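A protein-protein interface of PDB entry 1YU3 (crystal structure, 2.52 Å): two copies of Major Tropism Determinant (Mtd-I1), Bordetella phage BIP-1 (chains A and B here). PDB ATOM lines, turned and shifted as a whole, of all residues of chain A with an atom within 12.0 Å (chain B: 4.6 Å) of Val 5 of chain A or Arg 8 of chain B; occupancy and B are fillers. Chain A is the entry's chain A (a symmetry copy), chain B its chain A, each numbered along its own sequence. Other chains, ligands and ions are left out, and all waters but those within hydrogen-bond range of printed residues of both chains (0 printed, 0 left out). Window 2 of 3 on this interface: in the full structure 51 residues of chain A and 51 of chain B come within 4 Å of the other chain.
Among the printed residues, merely in contact across the chains: Gln 6 of chain A with Arg 23 of chain B, Val 5 of chain A with Glu 24 of chain B, Val 34 of chain A with Ile 25 of chain B, Gly 9 of chain A with Arg 23 of chain B, Phe 7 of chain A with Ile 25 of chain B, Phe 7 of chain A with Phe 7 of chain B, Ile 25 of chain A with Ile 25 of chain B, Thr 29 of chain A with Arg 23 of chain B, Val 5 of chain A with Arg 23 of chain B and Val 27 of chain A with Arg 23 of chain B.
The backbone NH (N) of Val 27 of chain B lies within hydrogen-bond range of the backbone carbonyl oxygen (O) of Arg 8 of chain B (3.0 Å).
O of Arg 8 of chain A lies within hydrogen-bond range of N of Val 27 of chain A, at 3.0 Å.
The guanidinium group (NH1) of Arg 8 of chain B is in salt-bridge range of the side-chain carboxylate (OE2) of Glu 24 of chain B.
Val 5 of chain A touches just these residues of chain B: Arg 8, Arg 23 and Glu 24.
Of chain A, only Val 5 (2.7 Å) comes within 4 Å of Arg 8 of chain B.
Phe 7 of chain B touches just one residue of chain A: Phe 7 (3.6 Å).
No residue of chain A comes within 4 Å of Gly 9 of chain B.
Glu 24 of chain B touches just one residue of chain A: Val 5.
Ile 25 of chain B touches just these residues of chain A: Phe 7, Ile 25 and Val 34.
Thr 26 of chain B touches none of the printed residues of chain A.
No residue of chain A comes within 4 Å of Val 27 of chain B.
Of the printed residues of chain B, Gly 9 of chain A touches Arg 23 (3.6 Å).
Of the printed residues of chain B, Thr 29 of chain A touches Arg 23.
Arg 23 of chain A touches none of the printed residues of chain B.
The nearest residue of chain A that does not touch Arg 8 of chain B is Gln 6 of chain A (5.9 Å).
The guanidinium group (NH1) of Arg 8 of chain B sits close to the backbone NH (N) of Val 5 of chain A (2.7 Å).
The guanidinium group (NE) of Arg 23 of chain B lies within hydrogen-bond range of the backbone carbonyl oxygen (O) of Phe 7 of chain A (2.7 Å).
Hydrophobic or aromatic side chains of chain B that line the printed part of chain A: Phe 7 and Ile 25.
Of the 12 printed residues of chain A, 8 touch a printed residue of chain B.
Hydrophobic or aromatic side chains of chain A that line the printed part of chain B: Phe 7, Ile 25, Val 27 and Val 34.
Among the printed residues, no Asp or Glu carboxylate lies within 4 Å of a Lys or Arg side-chain nitrogen of the other chain.
Phe 7 of chain A touches its own counterpart, Phe 7 of chain B.
Phe 7 of chain A touches Arg 23 of chain B, but with the chains exchanged Arg 23 of chain A does not touch Phe 7 of chain B (9.4 Å).
Gly 9 of chain A touches Arg 23 of chain B, but with the chains exchanged Arg 23 of chain A does not touch Gly 9 of chain B (18.9 Å).
Val 27 of chain A touches Arg 23 of chain B, but with the chains exchanged Arg 23 of chain A does not touch Val 27 of chain B (14.5 Å).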
ATOM      1  N   VAL A   5      10.237   5.965  13.120  1.00  0.00           N
ATOM      2  CA  VAL A   5       9.311   6.596  12.133  1.00  0.00           C
ATOM      3  C   VAL A   5       9.774   8.005  11.738  1.00  0.00           C
ATOM      4  O   VAL A   5       9.841   8.916  12.577  1.00  0.00           O
ATOM      5  CB  VAL A   5       7.841   6.674  12.654  1.00  0.00           C
ATOM      6  CG1 VAL A   5       6.861   6.721  11.476  1.00  0.00           C
ATOM      7  CG2 VAL A   5       7.510   5.497  13.589  1.00  0.00           C
ATOM      8  N   GLN A   6      10.096   8.162  10.456  1.00  0.00           N
ATOM      9  CA  GLN A   6      10.430   9.462   9.878  1.00  0.00           C
ATOM     10  C   GLN A   6       9.297   9.898   8.965  1.00  0.00           C
ATOM     11  O   GLN A   6       8.869   9.142   8.090  1.00  0.00           O
ATOM     12  CB  GLN A   6      11.717   9.384   9.063  1.00  0.00           C
ATOM     13  CG  GLN A   6      12.909   8.795   9.793  1.00  0.00           C
ATOM     14  CD  GLN A   6      14.170   8.882   8.962  1.00  0.00           C
ATOM     15  OE1 GLN A   6      14.671   9.969   8.684  1.00  0.00           O
ATOM     16  NE2 GLN A   6      14.692   7.730   8.556  1.00  0.00           N
ATOM     17  N   PHE A   7       8.825  11.124   9.156  1.00  0.00           N
ATOM     18  CA  PHE A   7       7.682  11.627   8.403  1.00  0.00           C
ATOM     19  C   PHE A   7       8.079  12.262   7.089  1.00  0.00           C
ATOM     20  O   PHE A   7       9.221  12.693   6.924  1.00  0.00           O
ATOM     21  CB  PHE A   7       6.894  12.614   9.260  1.00  0.00           C
ATOM     22  CG  PHE A   7       6.192  11.965  10.395  1.00  0.00           C
ATOM     23  CD1 PHE A   7       4.922  11.436  10.222  1.00  0.00           C
ATOM     24  CD2 PHE A   7       6.815  11.831  11.623  1.00  0.00           C
ATOM     25  CE1 PHE A   7       4.269  10.804  11.267  1.00  0.00           C
ATOM     26  CE2 PHE A   7       6.176  11.197  12.675  1.00  0.00           C
ATOM     27  CZ  PHE A   7       4.898  10.684  12.499  1.00  0.00           C
ATOM     28  N   ARG A   8       7.130  12.309   6.151  1.00  0.00           N
ATOM     29  CA  ARG A   8       7.308  13.087   4.930  1.00  0.00           C
ATOM     30  C   ARG A   8       7.628  14.514   5.360  1.00  0.00           C
ATOM     31  O   ARG A   8       6.980  15.073   6.251  1.00  0.00           O
ATOM     32  CB  ARG A   8       6.063  13.043   4.022  1.00  0.00           C
ATOM     33  CG  ARG A   8       5.804  11.695   3.318  1.00  0.00           C
ATOM     34  CD  ARG A   8       4.672  10.901   3.999  1.00  0.00           C
ATOM     35  NE  ARG A   8       4.440   9.575   3.403  1.00  0.00           N
ATOM     36  CZ  ARG A   8       3.322   8.853   3.548  1.00  0.00           C
ATOM     37  NH1 ARG A   8       2.298   9.317   4.262  1.00  0.00           N
ATOM     38  NH2 ARG A   8       3.218   7.660   2.967  1.00  0.00           N
ATOM     39  N   GLY A   9       8.665  15.081   4.765  1.00  0.00           N
ATOM     40  CA  GLY A   9       9.081  16.423   5.120  1.00  0.00           C
ATOM     41  C   GLY A   9       9.589  17.171   3.920  1.00  0.00           C
ATOM     42  O   GLY A   9       9.967  16.570   2.914  1.00  0.00           O
ATOM     43  N   ARG A  23      -5.557  14.702   8.422  1.00  0.00           N
ATOM     44  CA  ARG A  23      -4.939  14.161   9.632  1.00  0.00           C
ATOM     45  C   ARG A  23      -3.558  13.538   9.351  1.00  0.00           C
ATOM     46  O   ARG A  23      -3.087  12.670  10.087  1.00  0.00           O
ATOM     47  CB  ARG A  23      -5.888  13.179  10.349  1.00  0.00           C
ATOM     48  CG  ARG A  23      -7.345  13.682  10.452  1.00  0.00           C
ATOM     49  CD  ARG A  23      -8.284  12.708  11.161  1.00  0.00           C
ATOM     50  NE  ARG A  23      -8.065  11.332  10.733  1.00  0.00           N
ATOM     51  CZ  ARG A  23      -8.549  10.804   9.614  1.00  0.00           C
ATOM     52  NH1 ARG A  23      -9.301  11.531   8.800  1.00  0.00           N
ATOM     53  NH2 ARG A  23      -8.277   9.546   9.307  1.00  0.00           N
ATOM     54  N   GLU A  24      -2.915  13.994   8.275  1.00  0.00           N
ATOM     55  CA  GLU A  24      -1.512  13.674   8.026  1.00  0.00           C
ATOM     56  C   GLU A  24      -0.617  14.698   8.704  1.00  0.00           C
ATOM     57  O   GLU A  24      -0.948  15.885   8.780  1.00  0.00           O
ATOM     58  CB  GLU A  24      -1.198  13.630   6.526  1.00  0.00           C
ATOM     59  CG  GLU A  24       0.253  13.255   6.192  1.00  0.00           C
ATOM     60  CD  GLU A  24       0.548  13.211   4.692  1.00  0.00           C
ATOM     61  OE1 GLU A  24      -0.390  13.403   3.878  1.00  0.00           O
ATOM     62  OE2 GLU A  24       1.729  12.981   4.328  1.00  0.00           O
ATOM     63  N   ILE A  25       0.522  14.226   9.192  1.00  0.00           N
ATOM     64  CA  ILE A  25       1.532  15.086   9.784  1.00  0.00           C
ATOM     65  C   ILE A  25       2.786  15.052   8.916  1.00  0.00           C
ATOM     66  O   ILE A  25       3.299  13.974   8.606  1.00  0.00           O
ATOM     67  CB  ILE A  25       1.810  14.673  11.247  1.00  0.00           C
ATOM     68  CG1 ILE A  25       0.724  15.269  12.144  1.00  0.00           C
ATOM     69  CG2 ILE A  25       3.204  15.109  11.708  1.00  0.00           C
ATOM     70  CD1 ILE A  25       0.547  14.567  13.466  1.00  0.00           C
ATOM     71  N   THR A  26       3.237  16.230   8.488  1.00  0.00           N
ATOM     72  CA  THR A  26       4.522  16.365   7.816  1.00  0.00           C
ATOM     73  C   THR A  26       5.472  17.215   8.670  1.00  0.00           C
ATOM     74  O   THR A  26       5.050  17.811   9.668  1.00  0.00           O
ATOM     75  CB  THR A  26       4.393  16.991   6.396  1.00  0.00           C
ATOM     76  OG1 THR A  26       3.889  18.329   6.496  1.00  0.00           O
ATOM     77  CG2 THR A  26       3.509  16.148   5.482  1.00  0.00           C
ATOM     78  N   VAL A  27       6.749  17.259   8.284  1.00  0.00           N
ATOM     79  CA  VAL A  27       7.747  18.071   8.989  1.00  0.00           C
ATOM     80  C   VAL A  27       8.342  19.117   8.054  1.00  0.00           C
ATOM     81  O   VAL A  27       8.937  18.771   7.035  1.00  0.00           O
ATOM     82  CB  VAL A  27       8.893  17.204   9.587  1.00  0.00           C
ATOM     83  CG1 VAL A  27       9.953  18.080  10.254  1.00  0.00           C
ATOM     84  CG2 VAL A  27       8.340  16.194  10.580  1.00  0.00           C
ATOM     85  N   THR A  29      11.185  21.212   7.258  1.00  0.00           N
ATOM     86  CA  THR A  29      12.594  21.102   7.620  1.00  0.00           C
ATOM     87  C   THR A  29      13.299  22.450   7.715  1.00  0.00           C
ATOM     88  O   THR A  29      14.348  22.542   8.339  1.00  0.00           O
ATOM     89  CB  THR A  29      13.358  20.170   6.670  1.00  0.00           C
ATOM     90  OG1 THR A  29      13.127  20.581   5.319  1.00  0.00           O
ATOM     91  CG2 THR A  29      12.893  18.726   6.849  1.00  0.00           C
ATOM     92  N   VAL A  34       6.215  20.654  13.180  1.00  0.00           N
ATOM     93  CA  VAL A  34       5.218  19.780  12.598  1.00  0.00           C
ATOM     94  C   VAL A  34       4.246  20.606  11.751  1.00  0.00           C
ATOM     95  O   VAL A  34       3.925  21.753  12.087  1.00  0.00           O
ATOM     96  CB  VAL A  34       4.490  18.996  13.722  1.00  0.00           C
ATOM     97  CG1 VAL A  34       3.211  18.357  13.241  1.00  0.00           C
ATOM     98  CG2 VAL A  34       5.424  17.944  14.302  1.00  0.00           C
ATOM     99  N   GLN B   6       1.997   4.497  19.144  1.00  0.00           N
ATOM    100  CA  GLN B   6       2.665   5.134  20.276  1.00  0.00           C
ATOM    101  C   GLN B   6       4.102   5.442  19.888  1.00  0.00           C
ATOM    102  O   GLN B   6       4.823   4.566  19.407  1.00  0.00           O
ATOM    103  CB  GLN B   6       2.671   4.217  21.495  1.00  0.00           C
ATOM    104  CG  GLN B   6       1.315   3.677  21.903  1.00  0.00           C
ATOM    105  CD  GLN B   6       1.392   2.892  23.195  1.00  0.00           C
ATOM    106  OE1 GLN B   6       1.672   3.447  24.255  1.00  0.00           O
ATOM    107  NE2 GLN B   6       1.146   1.591  23.112  1.00  0.00           N
ATOM    108  N   PHE B   7       4.521   6.681  20.114  1.00  0.00           N
ATOM    109  CA  PHE B   7       5.848   7.124  19.705  1.00  0.00           C
ATOM    110  C   PHE B   7       6.906   6.851  20.752  1.00  0.00           C
ATOM    111  O   PHE B   7       6.591   6.706  21.934  1.00  0.00           O
ATOM    112  CB  PHE B   7       5.813   8.609  19.355  1.00  0.00           C
ATOM    113  CG  PHE B   7       5.051   8.893  18.114  1.00  0.00           C
ATOM    114  CD1 PHE B   7       5.679   8.840  16.879  1.00  0.00           C
ATOM    115  CD2 PHE B   7       3.694   9.161  18.167  1.00  0.00           C
ATOM    116  CE1 PHE B   7       4.971   9.076  15.712  1.00  0.00           C
ATOM    117  CE2 PHE B   7       2.973   9.395  17.008  1.00  0.00           C
ATOM    118  CZ  PHE B   7       3.613   9.355  15.777  1.00  0.00           C
ATOM    119  N   ARG B   8       8.162   6.770  20.308  1.00  0.00           N
ATOM    120  CA  ARG B   8       9.292   6.733  21.230  1.00  0.00           C
ATOM    121  C   ARG B   8       9.175   7.967  22.117  1.00  0.00           C
ATOM    122  O   ARG B   8       8.922   9.077  21.639  1.00  0.00           O
ATOM    123  CB  ARG B   8      10.646   6.700  20.495  1.00  0.00           C
ATOM    124  CG  ARG B   8      10.980   5.375  19.779  1.00  0.00           C
ATOM    125  CD  ARG B   8      10.764   5.477  18.256  1.00  0.00           C
ATOM    126  NE  ARG B   8      11.002   4.212  17.541  1.00  0.00           N
ATOM    127  CZ  ARG B   8      11.240   4.105  16.228  1.00  0.00           C
ATOM    128  NH1 ARG B   8      11.294   5.187  15.454  1.00  0.00           N
ATOM    129  NH2 ARG B   8      11.439   2.908  15.681  1.00  0.00           N
ATOM    130  N   GLY B   9       9.304   7.761  23.418  1.00  0.00           N
ATOM    131  CA  GLY B   9       9.178   8.856  24.359  1.00  0.00           C
ATOM    132  C   GLY B   9      10.117   8.688  25.520  1.00  0.00           C
ATOM    133  O   GLY B   9      10.587   7.585  25.797  1.00  0.00           O
ATOM    134  N   ARG B  23      13.290  14.306  10.886  1.00  0.00           N
ATOM    135  CA  ARG B  23      11.838  14.242  10.723  1.00  0.00           C
ATOM    136  C   ARG B  23      11.207  13.116  11.565  1.00  0.00           C
ATOM    137  O   ARG B  23      10.127  12.613  11.252  1.00  0.00           O
ATOM    138  CB  ARG B  23      11.451  14.146   9.233  1.00  0.00           C
ATOM    139  CG  ARG B  23      12.232  15.117   8.320  1.00  0.00           C
ATOM    140  CD  ARG B  23      11.848  15.019   6.845  1.00  0.00           C
ATOM    141  NE  ARG B  23      11.709  13.635   6.410  1.00  0.00           N
ATOM    142  CZ  ARG B  23      12.723  12.842   6.080  1.00  0.00           C
ATOM    143  NH1 ARG B  23      13.967  13.294   6.119  1.00  0.00           N
ATOM    144  NH2 ARG B  23      12.490  11.592   5.713  1.00  0.00           N
ATOM    145  N   GLU B  24      11.897  12.728  12.638  1.00  0.00           N
ATOM    146  CA  GLU B  24      11.312  11.851  13.650  1.00  0.00           C
ATOM    147  C   GLU B  24      10.593  12.679  14.702  1.00  0.00           C
ATOM    148  O   GLU B  24      11.025  13.781  15.053  1.00  0.00           O
ATOM    149  CB  GLU B  24      12.376  10.975  14.323  1.00  0.00           C
ATOM    150  CG  GLU B  24      11.822   9.996  15.369  1.00  0.00           C
ATOM    151  CD  GLU B  24      12.894   9.127  16.027  1.00  0.00           C
ATOM    152  OE1 GLU B  24      14.083   9.218  15.632  1.00  0.00           O
ATOM    153  OE2 GLU B  24      12.540   8.345  16.945  1.00  0.00           O
ATOM    154  N   ILE B  25       9.494  12.134  15.204  1.00  0.00           N
ATOM    155  CA  ILE B  25       8.743  12.747  16.285  1.00  0.00           C
ATOM    156  C   ILE B  25       8.820  11.851  17.517  1.00  0.00           C
ATOM    157  O   ILE B  25       8.520  10.657  17.438  1.00  0.00           O
ATOM    158  CB  ILE B  25       7.287  13.030  15.845  1.00  0.00           C
ATOM    159  CG1 ILE B  25       7.258  14.329  15.039  1.00  0.00           C
ATOM    160  CG2 ILE B  25       6.334  13.105  17.043  1.00  0.00           C
ATOM    161  CD1 ILE B  25       6.066  14.475  14.128  1.00  0.00           C
ATOM    162  N   THR B  26       9.274  12.422  18.631  1.00  0.00           N
ATOM    163  CA  THR B  26       9.222  11.745  19.920  1.00  0.00           C
ATOM    164  C   THR B  26       8.282  12.500  20.870  1.00  0.00           C
ATOM    165  O   THR B  26       7.839  13.611  20.558  1.00  0.00           O
ATOM    166  CB  THR B  26      10.625  11.600  20.578  1.00  0.00           C
ATOM    167  OG1 THR B  26      11.166  12.896  20.866  1.00  0.00           O
ATOM    168  CG2 THR B  26      11.583  10.798  19.701  1.00  0.00           C
ATOM    169  N   VAL B  27       7.975  11.893  22.018  1.00  0.00           N
ATOM    170  CA  VAL B  27       7.124  12.527  23.030  1.00  0.00           C
ATOM    171  C   VAL B  27       7.885  12.695  24.340  1.00  0.00           C
ATOM    172  O   VAL B  27       8.328  11.711  24.930  1.00  0.00           O
ATOM    173  CB  VAL B  27       5.820  11.718  23.293  1.00  0.00           C
ATOM    174  CG1 VAL B  27       4.987  12.363  24.400  1.00  0.00           C
ATOM    175  CG2 VAL B  27       5.001  11.591  22.018  1.00  0.00           C
